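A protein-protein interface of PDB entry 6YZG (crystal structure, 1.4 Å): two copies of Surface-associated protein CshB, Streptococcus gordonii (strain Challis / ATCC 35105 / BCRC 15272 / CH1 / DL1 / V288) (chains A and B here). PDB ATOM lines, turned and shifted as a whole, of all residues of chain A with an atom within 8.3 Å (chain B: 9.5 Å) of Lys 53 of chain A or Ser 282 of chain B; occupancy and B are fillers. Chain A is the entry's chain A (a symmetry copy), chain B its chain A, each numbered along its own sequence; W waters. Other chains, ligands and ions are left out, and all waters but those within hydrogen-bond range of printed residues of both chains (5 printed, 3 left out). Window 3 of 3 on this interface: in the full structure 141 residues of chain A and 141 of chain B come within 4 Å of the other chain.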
ATOM      1  N   THR A  48      -9.308 -13.528  16.161  1.00  0.00           N
ATOM      2  CA  THR A  48      -9.385 -12.370  17.089  1.00  0.00           C
ATOM      3  C   THR A  48     -10.143 -11.170  16.516  1.00  0.00           C
ATOM      4  O   THR A  48     -10.212 -11.022  15.346  1.00  0.00           O
ATOM      5  CB  THR A  48      -7.987 -11.889  17.508  1.00  0.00           C
ATOM      6  OG1 THR A  48      -7.291 -11.375  16.371  1.00  0.00           O
ATOM      7  CG2 THR A  48      -7.157 -12.982  18.137  1.00  0.00           C
ATOM      8  N   GLU A  49     -10.641 -10.325  17.407  1.00  0.00           N
ATOM      9  CA  GLU A  49     -11.301  -9.059  16.998  1.00  0.00           C
ATOM     10  C   GLU A  49     -10.259  -8.136  16.354  1.00  0.00           C
ATOM     11  O   GLU A  49     -10.614  -7.393  15.527  1.00  0.00           O
ATOM     12  CB  GLU A  49     -11.956  -8.366  18.190  1.00  0.00           C
ATOM     13  CG  GLU A  49     -13.095  -9.163  18.753  1.00  0.00           C
ATOM     14  CD  GLU A  49     -14.464  -8.987  18.134  1.00  0.00           C
ATOM     15  OE1 GLU A  49     -14.665  -8.041  17.391  1.00  0.00           O
ATOM     16  OE2 GLU A  49     -15.351  -9.793  18.477  1.00  0.00           O
ATOM     17  N   ILE A  50      -8.999  -8.231  16.780  1.00  0.00           N
ATOM     18  CA  ILE A  50      -7.910  -7.463  16.147  1.00  0.00           C
ATOM     19  C   ILE A  50      -7.906  -7.768  14.636  1.00  0.00           C
ATOM     20  O   ILE A  50      -7.891  -6.884  13.795  1.00  0.00           O
ATOM     21  CB  ILE A  50      -6.548  -7.738  16.798  1.00  0.00           C
ATOM     22  CG1 ILE A  50      -6.513  -7.395  18.301  1.00  0.00           C
ATOM     23  CG2 ILE A  50      -5.480  -7.039  16.000  1.00  0.00           C
ATOM     24  CD1 ILE A  50      -5.515  -8.248  19.016  1.00  0.00           C
ATOM     25  N   TYR A  51      -7.856  -9.057  14.319  1.00  0.00           N
ATOM     26  CA  TYR A  51      -7.801  -9.501  12.917  1.00  0.00           C
ATOM     27  C   TYR A  51      -9.140  -9.141  12.182  1.00  0.00           C
ATOM     28  O   TYR A  51      -9.037  -8.661  11.056  1.00  0.00           O
ATOM     29  CB  TYR A  51      -7.547 -11.015  12.903  1.00  0.00           C
ATOM     30  CG  TYR A  51      -7.452 -11.580  11.517  1.00  0.00           C
ATOM     31  CD1 TYR A  51      -6.260 -11.599  10.791  1.00  0.00           C
ATOM     32  CD2 TYR A  51      -8.603 -12.095  10.908  1.00  0.00           C
ATOM     33  CE1 TYR A  51      -6.169 -12.167   9.546  1.00  0.00           C
ATOM     34  CE2 TYR A  51      -8.519 -12.660   9.652  1.00  0.00           C
ATOM     35  CZ  TYR A  51      -7.310 -12.713   8.986  1.00  0.00           C
ATOM     36  OH  TYR A  51      -7.283 -13.235   7.696  1.00  0.00           O
ATOM     37  N   LYS A  52     -10.243  -9.351  12.870  1.00  0.00           N
ATOM     38  CA  LYS A  52     -11.599  -8.973  12.312  1.00  0.00           C
ATOM     39  C   LYS A  52     -11.532  -7.534  11.830  1.00  0.00           C
ATOM     40  O   LYS A  52     -11.900  -7.233  10.654  1.00  0.00           O
ATOM     41  CB  LYS A  52     -12.672  -9.178  13.358  1.00  0.00           C
ATOM     42  CG  LYS A  52     -14.049  -8.751  12.865  1.00  0.00           C
ATOM     43  CD  LYS A  52     -15.050  -8.702  13.934  1.00  0.00           C
ATOM     44  CE  LYS A  52     -16.447  -8.574  13.339  1.00  0.00           C
ATOM     45  NZ  LYS A  52     -17.425  -8.297  14.417  1.00  0.00           N
ATOM     46  N   LYS A  53     -11.007  -6.634  12.653  1.00  0.00           N
ATOM     47  CA  LYS A  53     -10.951  -5.208  12.256  1.00  0.00           C
ATOM     48  C   LYS A  53      -9.962  -4.948  11.118  1.00  0.00           C
ATOM     49  O   LYS A  53     -10.210  -4.078  10.328  1.00  0.00           O
ATOM     50  CB  LYS A  53     -10.742  -4.327  13.487  1.00  0.00           C
ATOM     51  CG  LYS A  53     -11.882  -4.408  14.496  1.00  0.00           C
ATOM     52  CD  LYS A  53     -11.639  -3.728  15.810  1.00  0.00           C
ATOM     53  CE  LYS A  53     -12.575  -4.186  16.911  1.00  0.00           C
ATOM     54  NZ  LYS A  53     -12.235  -3.555  18.208  1.00  0.00           N
ATOM     55  N   ARG A  54      -8.854  -5.672  11.070  1.00  0.00           N
ATOM     56  CA  ARG A  54      -7.887  -5.478  10.005  1.00  0.00           C
ATOM     57  C   ARG A  54      -8.463  -5.924   8.651  1.00  0.00           C
ATOM     58  O   ARG A  54      -8.074  -5.324   7.655  1.00  0.00           O
ATOM     59  CB  ARG A  54      -6.572  -6.221  10.270  1.00  0.00           C
ATOM     60  CG  ARG A  54      -5.851  -5.684  11.509  1.00  0.00           C
ATOM     61  CD  ARG A  54      -4.595  -6.466  11.683  1.00  0.00           C
ATOM     62  NE  ARG A  54      -3.754  -5.983  12.804  1.00  0.00           N
ATOM     63  CZ  ARG A  54      -2.590  -6.509  13.113  1.00  0.00           C
ATOM     64  NH1 ARG A  54      -2.121  -7.572  12.481  1.00  0.00           N
ATOM     65  NH2 ARG A  54      -1.901  -6.089  14.180  1.00  0.00           N
ATOM     66  N   VAL A  55      -9.311  -6.953   8.615  1.00  0.00           N
ATOM     67  CA  VAL A  55      -9.803  -7.435   7.278  1.00  0.00           C
ATOM     68  C   VAL A  55     -11.161  -6.786   6.957  1.00  0.00           C
ATOM     69  O   VAL A  55     -11.611  -6.990   5.804  1.00  0.00           O
ATOM     70  CB  VAL A  55      -9.905  -8.976   7.182  1.00  0.00           C
ATOM     71  CG1 VAL A  55      -8.554  -9.634   7.257  1.00  0.00           C
ATOM     72  CG2 VAL A  55     -10.840  -9.566   8.200  1.00  0.00           C
ATOM     73  N   ALA A  56     -11.789  -6.069   7.866  1.00  0.00           N
ATOM     74  CA  ALA A  56     -13.146  -5.515   7.616  1.00  0.00           C
ATOM     75  C   ALA A  56     -13.110  -4.684   6.331  1.00  0.00           C
ATOM     76  O   ALA A  56     -12.214  -3.819   6.173  1.00  0.00           O
ATOM     77  CB  ALA A  56     -13.548  -4.650   8.771  1.00  0.00           C
ATOM     78  N   GLY A  57     -14.103  -4.929   5.466  1.00  0.00           N
ATOM     79  CA  GLY A  57     -14.283  -4.059   4.289  1.00  0.00           C
ATOM     80  C   GLY A  57     -13.304  -4.360   3.184  1.00  0.00           C
ATOM     81  O   GLY A  57     -13.246  -3.576   2.208  1.00  0.00           O
ATOM     82  N   THR A  58     -12.574  -5.470   3.261  1.00  0.00           N
ATOM     83  CA  THR A  58     -11.655  -5.931   2.206  1.00  0.00           C
ATOM     84  C   THR A  58     -12.157  -7.239   1.624  1.00  0.00           C
ATOM     85  O   THR A  58     -13.115  -7.887   2.152  1.00  0.00           O
ATOM     86  CB  THR A  58     -10.216  -6.149   2.726  1.00  0.00           C
ATOM     87  OG1 THR A  58     -10.217  -7.379   3.476  1.00  0.00           O
ATOM     88  CG2 THR A  58      -9.681  -5.016   3.570  1.00  0.00           C
ATOM     89  N   GLU A  61     -12.356 -10.216   4.030  1.00  0.00           N
ATOM     90  CA  GLU A  61     -13.150 -10.090   5.252  1.00  0.00           C
ATOM     91  C   GLU A  61     -13.647 -11.454   5.699  1.00  0.00           C
ATOM     92  O   GLU A  61     -13.738 -11.712   6.912  1.00  0.00           O
ATOM     93  CB  GLU A  61     -14.258  -9.055   5.010  1.00  0.00           C
ATOM     94  CG  GLU A  61     -15.269  -8.987   6.110  1.00  0.00           C
ATOM     95  CD  GLU A  61     -16.373  -7.970   5.809  1.00  0.00           C
ATOM     96  OE1 GLU A  61     -16.082  -6.775   5.716  1.00  0.00           O
ATOM     97  OE2 GLU A  61     -17.521  -8.395   5.597  1.00  0.00           O
ATOM     98  N   TYR A  64     -11.926 -13.897   8.556  1.00  0.00           N
ATOM     99  CA  TYR A  64     -12.136 -13.840  10.014  1.00  0.00           C
ATOM    100  C   TYR A  64     -12.971 -15.008  10.454  1.00  0.00           C
ATOM    101  O   TYR A  64     -14.115 -15.189   9.915  1.00  0.00           O
ATOM    102  CB  TYR A  64     -12.752 -12.518  10.437  1.00  0.00           C
ATOM    103  CG  TYR A  64     -13.301 -12.528  11.846  1.00  0.00           C
ATOM    104  CD1 TYR A  64     -12.486 -12.719  12.953  1.00  0.00           C
ATOM    105  CD2 TYR A  64     -14.652 -12.331  12.070  1.00  0.00           C
ATOM    106  CE1 TYR A  64     -13.001 -12.715  14.236  1.00  0.00           C
ATOM    107  CE2 TYR A  64     -15.170 -12.277  13.343  1.00  0.00           C
ATOM    108  CZ  TYR A  64     -14.334 -12.430  14.434  1.00  0.00           C
ATOM    109  OH  TYR A  64     -14.795 -12.443  15.724  1.00  0.00           O
ATOM    110  N   THR A 158      -1.617  -7.592  24.712  1.00  0.00           N
ATOM    111  CA  THR A 158      -1.747  -7.275  26.133  1.00  0.00           C
ATOM    112  C   THR A 158      -3.016  -6.432  26.357  1.00  0.00           C
ATOM    113  O   THR A 158      -3.424  -5.680  25.463  1.00  0.00           O
ATOM    114  CB  THR A 158      -0.526  -6.488  26.634  1.00  0.00           C
ATOM    115  OG1 THR A 158      -0.686  -6.240  28.031  1.00  0.00           O
ATOM    116  CG2 THR A 158      -0.275  -5.185  25.877  1.00  0.00           C
ATOM    117  N   ASN A 159      -3.586  -6.508  27.556  1.00  0.00           N
ATOM    118  CA  ASN A 159      -4.588  -5.531  28.001  1.00  0.00           C
ATOM    119  C   ASN A 159      -3.986  -4.612  29.052  1.00  0.00           C
ATOM    120  O   ASN A 159      -4.730  -3.811  29.647  1.00  0.00           O
ATOM    121  CB  ASN A 159      -5.886  -6.209  28.474  1.00  0.00           C
ATOM    122  CG  ASN A 159      -5.742  -6.811  29.818  1.00  0.00           C
ATOM    123  OD1 ASN A 159      -4.650  -6.971  30.360  1.00  0.00           O
ATOM    124  ND2 ASN A 159      -6.873  -7.221  30.392  1.00  0.00           N
ATOM    125  N   LYS A 209      -2.483  -9.452   6.734  1.00  0.00           N
ATOM    126  CA  LYS A 209      -3.120  -8.789   7.902  1.00  0.00           C
ATOM    127  C   LYS A 209      -2.641  -9.452   9.210  1.00  0.00           C
ATOM    128  O   LYS A 209      -3.127  -9.040  10.268  1.00  0.00           O
ATOM    129  CB  LYS A 209      -4.635  -8.674   7.783  1.00  0.00           C
ATOM    130  CG  LYS A 209      -5.054  -7.828   6.578  1.00  0.00           C
ATOM    131  CD  LYS A 209      -4.366  -6.466   6.568  1.00  0.00           C
ATOM    132  CE  LYS A 209      -4.685  -5.593   5.358  1.00  0.00           C
ATOM    133  NZ  LYS A 209      -6.107  -5.193   5.342  1.00  0.00           N
ATOM    134  N   GLN A 223      -1.003  -2.146  21.924  1.00  0.00           N
ATOM    135  CA  GLN A 223      -1.229  -3.412  22.642  1.00  0.00           C
ATOM    136  C   GLN A 223      -0.962  -4.628  21.746  1.00  0.00           C
ATOM    137  O   GLN A 223      -1.202  -5.757  22.226  1.00  0.00           O
ATOM    138  CB  GLN A 223      -2.614  -3.440  23.290  1.00  0.00           C
ATOM    139  CG  GLN A 223      -2.752  -2.488  24.454  1.00  0.00           C
ATOM    140  CD  GLN A 223      -4.087  -2.480  25.152  1.00  0.00           C
ATOM    141  OE1 GLN A 223      -4.161  -2.363  26.405  1.00  0.00           O
ATOM    142  NE2 GLN A 223      -5.134  -2.573  24.401  1.00  0.00           N
ATOM    143  N   GLU B 276     -10.507  -2.278  36.063  1.00  0.00           N
ATOM    144  CA  GLU B 276     -11.447  -2.920  35.098  1.00  0.00           C
ATOM    145  C   GLU B 276     -11.735  -1.968  33.926  1.00  0.00           C
ATOM    146  O   GLU B 276     -11.814  -2.460  32.763  1.00  0.00           O
ATOM    147  CB  GLU B 276     -12.714  -3.374  35.835  1.00  0.00           C
ATOM    148  CG  GLU B 276     -13.969  -3.490  34.966  1.00  0.00           C
ATOM    149  CD  GLU B 276     -14.280  -4.850  34.354  1.00  0.00           C
ATOM    150  OE1 GLU B 276     -15.340  -4.968  33.692  1.00  0.00           O
ATOM    151  OE2 GLU B 276     -13.474  -5.789  34.531  1.00  0.00           O
ATOM    152  N   ALA B 277     -11.880  -0.658  34.176  1.00  0.00           N
ATOM    153  CA  ALA B 277     -12.159   0.362  33.139  1.00  0.00           C
ATOM    154  C   ALA B 277     -11.075   0.313  32.045  1.00  0.00           C
ATOM    155  O   ALA B 277     -11.404   0.267  30.827  1.00  0.00           O
ATOM    156  CB  ALA B 277     -12.228   1.727  33.801  1.00  0.00           C
ATOM    157  N   PHE B 278      -9.809   0.310  32.452  1.00  0.00           N
ATOM    158  CA  PHE B 278      -8.644   0.190  31.535  1.00  0.00           C
ATOM    159  C   PHE B 278      -8.635  -1.202  30.878  1.00  0.00           C
ATOM    160  O   PHE B 278      -8.480  -1.340  29.648  1.00  0.00           O
ATOM    161  CB  PHE B 278      -7.349   0.431  32.326  1.00  0.00           C
ATOM    162  CG  PHE B 278      -6.115   0.423  31.467  1.00  0.00           C
ATOM    163  CD1 PHE B 278      -5.797   1.512  30.671  1.00  0.00           C
ATOM    164  CD2 PHE B 278      -5.263  -0.663  31.465  1.00  0.00           C
ATOM    165  CE1 PHE B 278      -4.662   1.505  29.874  1.00  0.00           C
ATOM    166  CE2 PHE B 278      -4.139  -0.674  30.653  1.00  0.00           C
ATOM    167  CZ  PHE B 278      -3.846   0.394  29.854  1.00  0.00           C
ATOM    168  N   HIS B 279      -8.730  -2.250  31.692  1.00  0.00           N
ATOM    169  CA  HIS B 279      -8.569  -3.639  31.200  1.00  0.00           C
ATOM    170  C   HIS B 279      -9.616  -4.014  30.154  1.00  0.00           C
ATOM    171  O   HIS B 279      -9.288  -4.911  29.323  1.00  0.00           O
ATOM    172  CB  HIS B 279      -8.635  -4.655  32.324  1.00  0.00           C
ATOM    173  CG  HIS B 279      -7.406  -4.684  33.155  1.00  0.00           C
ATOM    174  ND1 HIS B 279      -7.434  -5.077  34.486  1.00  0.00           N
ATOM    175  CD2 HIS B 279      -6.116  -4.436  32.833  1.00  0.00           C
ATOM    176  CE1 HIS B 279      -6.195  -5.055  34.970  1.00  0.00           C
ATOM    177  NE2 HIS B 279      -5.358  -4.687  33.952  1.00  0.00           N
ATOM    178  N   THR B 280     -10.832  -3.444  30.205  1.00  0.00           N
ATOM    179  CA  THR B 280     -11.949  -3.884  29.316  1.00  0.00           C
ATOM    180  C   THR B 280     -12.034  -3.070  28.015  1.00  0.00           C
ATOM    181  O   THR B 280     -12.928  -3.369  27.228  1.00  0.00           O
ATOM    182  CB  THR B 280     -13.301  -3.855  30.036  1.00  0.00           C
ATOM    183  OG1 THR B 280     -13.425  -2.567  30.627  1.00  0.00           O
ATOM    184  CG2 THR B 280     -13.396  -4.919  31.096  1.00  0.00           C
ATOM    185  N   ILE B 281     -11.186  -2.061  27.801  1.00  0.00           N
ATOM    186  CA  ILE B 281     -11.161  -1.313  26.509  1.00  0.00           C
ATOM    187  C   ILE B 281     -10.746  -2.346  25.451  1.00  0.00           C
ATOM    188  O   ILE B 281      -9.937  -3.220  25.757  1.00  0.00           O
ATOM    189  CB  ILE B 281     -10.226  -0.098  26.598  1.00  0.00           C
ATOM    190  CG1 ILE B 281     -10.659   0.824  27.751  1.00  0.00           C
ATOM    191  CG2 ILE B 281     -10.175   0.632  25.264  1.00  0.00           C
ATOM    192  CD1 ILE B 281      -9.744   1.989  28.024  1.00  0.00           C
ATOM    193  N   SER B 282     -11.308  -2.321  24.245  1.00  0.00           N
ATOM    194  CA  SER B 282     -10.946  -3.294  23.193  1.00  0.00           C
ATOM    195  C   SER B 282      -9.434  -3.192  22.990  1.00  0.00           C
ATOM    196  O   SER B 282      -8.938  -2.062  23.136  1.00  0.00           O
ATOM    197  CB  SER B 282     -11.686  -3.012  21.922  1.00  0.00           C
ATOM    198  OG  SER B 282     -11.574  -1.647  21.596  1.00  0.00           O
ATOM    199  N   THR B 283      -8.795  -4.288  22.592  1.00  0.00           N
ATOM    200  CA  THR B 283      -7.328  -4.317  22.305  1.00  0.00           C
ATOM    201  C   THR B 283      -7.004  -3.157  21.362  1.00  0.00           C
ATOM    202  O   THR B 283      -7.668  -3.000  20.271  1.00  0.00           O
ATOM    203  CB  THR B 283      -6.806  -5.606  21.694  1.00  0.00           C
ATOM    204  OG1 THR B 283      -7.139  -6.702  22.568  1.00  0.00           O
ATOM    205  CG2 THR B 283      -5.303  -5.585  21.484  1.00  0.00           C
ATOM    206  N   ARG B 284      -6.023  -2.322  21.707  1.00  0.00           N
ATOM    207  CA  ARG B 284      -5.653  -1.160  20.902  1.00  0.00           C
ATOM    208  C   ARG B 284      -4.565  -1.604  19.896  1.00  0.00           C
ATOM    209  O   ARG B 284      -3.402  -1.862  20.240  1.00  0.00           O
ATOM    210  CB  ARG B 284      -5.177  -0.005  21.773  1.00  0.00           C
ATOM    211  CG  ARG B 284      -4.808   1.233  20.971  1.00  0.00           C
ATOM    212  CD  ARG B 284      -4.621   2.497  21.831  1.00  0.00           C
ATOM    213  NE  ARG B 284      -3.670   2.194  22.850  1.00  0.00           N
ATOM    214  CZ  ARG B 284      -2.374   2.285  22.713  1.00  0.00           C
ATOM    215  NH1 ARG B 284      -1.625   1.898  23.727  1.00  0.00           N
ATOM    216  NH2 ARG B 284      -1.853   2.818  21.602  1.00  0.00           N
ATOM    217  N   ASP B 285      -4.955  -1.779  18.630  1.00  0.00           N
ATOM    218  CA  ASP B 285      -4.024  -2.134  17.578  1.00  0.00           C
ATOM    219  C   ASP B 285      -3.020  -1.030  17.333  1.00  0.00           C
ATOM    220  O   ASP B 285      -3.280   0.144  17.662  1.00  0.00           O
ATOM    221  CB  ASP B 285      -4.777  -2.472  16.291  1.00  0.00           C
ATOM    222  CG  ASP B 285      -4.071  -3.442  15.373  1.00  0.00           C
ATOM    223  OD1 ASP B 285      -2.918  -3.831  15.676  1.00  0.00           O
ATOM    224  OD2 ASP B 285      -4.710  -3.748  14.298  1.00  0.00           O
ATOM    225  N   THR B 288      -1.402   2.594  11.859  1.00  0.00           N
ATOM    226  CA  THR B 288      -0.895   2.426  10.498  1.00  0.00           C
ATOM    227  C   THR B 288       0.217   3.438  10.213  1.00  0.00           C
ATOM    228  O   THR B 288      -0.069   4.655  10.294  1.00  0.00           O
ATOM    229  CB  THR B 288      -2.083   2.480   9.535  1.00  0.00           C
ATOM    230  OG1 THR B 288      -2.978   1.401   9.852  1.00  0.00           O
ATOM    231  CG2 THR B 288      -1.572   2.402   8.117  1.00  0.00           C
HETATM  232  O   HOH W   1      -7.467  -4.165  26.184  1.00  0.00           O
HETATM  233  O   HOH W   2      -9.513  -4.826  18.930  1.00  0.00           O
HETATM  234  O   HOH W   3      -2.469   0.670  26.550  1.00  0.00           O
HETATM  235  O   HOH W   4      -7.395  -4.120  14.331  1.00  0.00           O
HETATM  236  O   HOH W   5      -7.126  -0.804  24.966  1.00  0.00           O
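Of chain B, only Ser 282 comes within 4 Å of Lys 53 of chain A. Ser 282 of chain B touches one residue of chain A. No residue of chain B comes within 4 Å of Ala 56 of chain A. Printed residues of chain B within 4 Å of Ile 50 of chain A: Thr 283 and Asp 285. Printed residues of chain A within 4 Å of Asp 285 of chain B: Ile 50 and Arg 54. Of the printed residues of chain A, Phe 278 of chain B touches Asn 159. Of the printed residues of chain B, Asn 159 of chain A touches Phe 278 (3.3 Å) and His 279 (3.5 Å). Of the printed residues of chain A, Arg 284 of chain B touches Gln 223. Glu 61 of chain A touches none of the printed residues of chain B. Ile 281 of chain B touches none of the printed residues of chain A. The nearest residue of chain A that does not touch Ser 282 of chain B is Gln 223 of chain A (4.04 Å). The nearest printed residue of chain A that does not touch Thr 283 of chain B is Thr 158 of chain A (4.4 Å).
Along chain B the printed residues that touch a printed residue of chain A span positions 278 to 285. Hydrophobic or aromatic side chains of chain A that line the printed part of chain B: Ile 50. Among the printed residues, 8 pairs touch across the chains. Among the printed residues, Asp or Glu carboxylates within 4 Å of a Lys or Arg side-chain nitrogen of the other chain: Arg 54 of chain A with Asp 285 of chain B.
No position is printed for both chains.
Water W1 lies within hydrogen-bond range of O of Ile 281 of chain B (2.7 Å) and NE2 of Gln 223 of chain A (3.3 Å). Water W4 lies within hydrogen-bond range of OD2 of Asp 285 of chain B (2.7 Å) and O of Ile 50 of chain A (2.9 Å). Water W5 bridges the side-chain amide nitrogen of Gln 223 of chain A (2.7 Å) and the backbone carbonyl oxygen of Ser 282 of chain B (2.9 Å). Water W2 bridges O of Thr 283 of chain B and NZ of Lys 53 of chain A. Water W3 lies within hydrogen-bond range of NH1 of Arg 284 of chain B (3.2 Å) and OE1 of Gln 223 of chain A (3.5 Å).
The side-chain carboxylate of Asp 285 of chain B is in salt-bridge range of the guanidinium group of Arg 54 of chain A, 2.9 Å away. The side-chain amide nitrogen of Gln 223 of chain A lies close to the backbone NH of Arg 284 of chain B, at 2.8 Å.
Thr 283 of chain B touches Ile 50 of chain A (CG2 to CD1, 3.6 Å). Ile 50 of chain A touches Asp 285 of chain B (CG2 to OD2, 3.8 Å). Lys 53 of chain A touches Ser 282 of chain B. Asn 159 of chain A touches Phe 278 of chain B. ND2 of Asn 159 of chain A touches O of His 279 of chain B, 3.5 Å away. NE2 of Gln 223 of chain A touches CA of Thr 283 of chain B (3.5 Å).
NH1 of Arg 54 of chain A sits at hydrogen-bond distance from O of Lys 209 of chain A, at 2.8 Å. O of Gln 223 of chain A is in hydrogen-bond range of N of Thr 158 of chain A.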
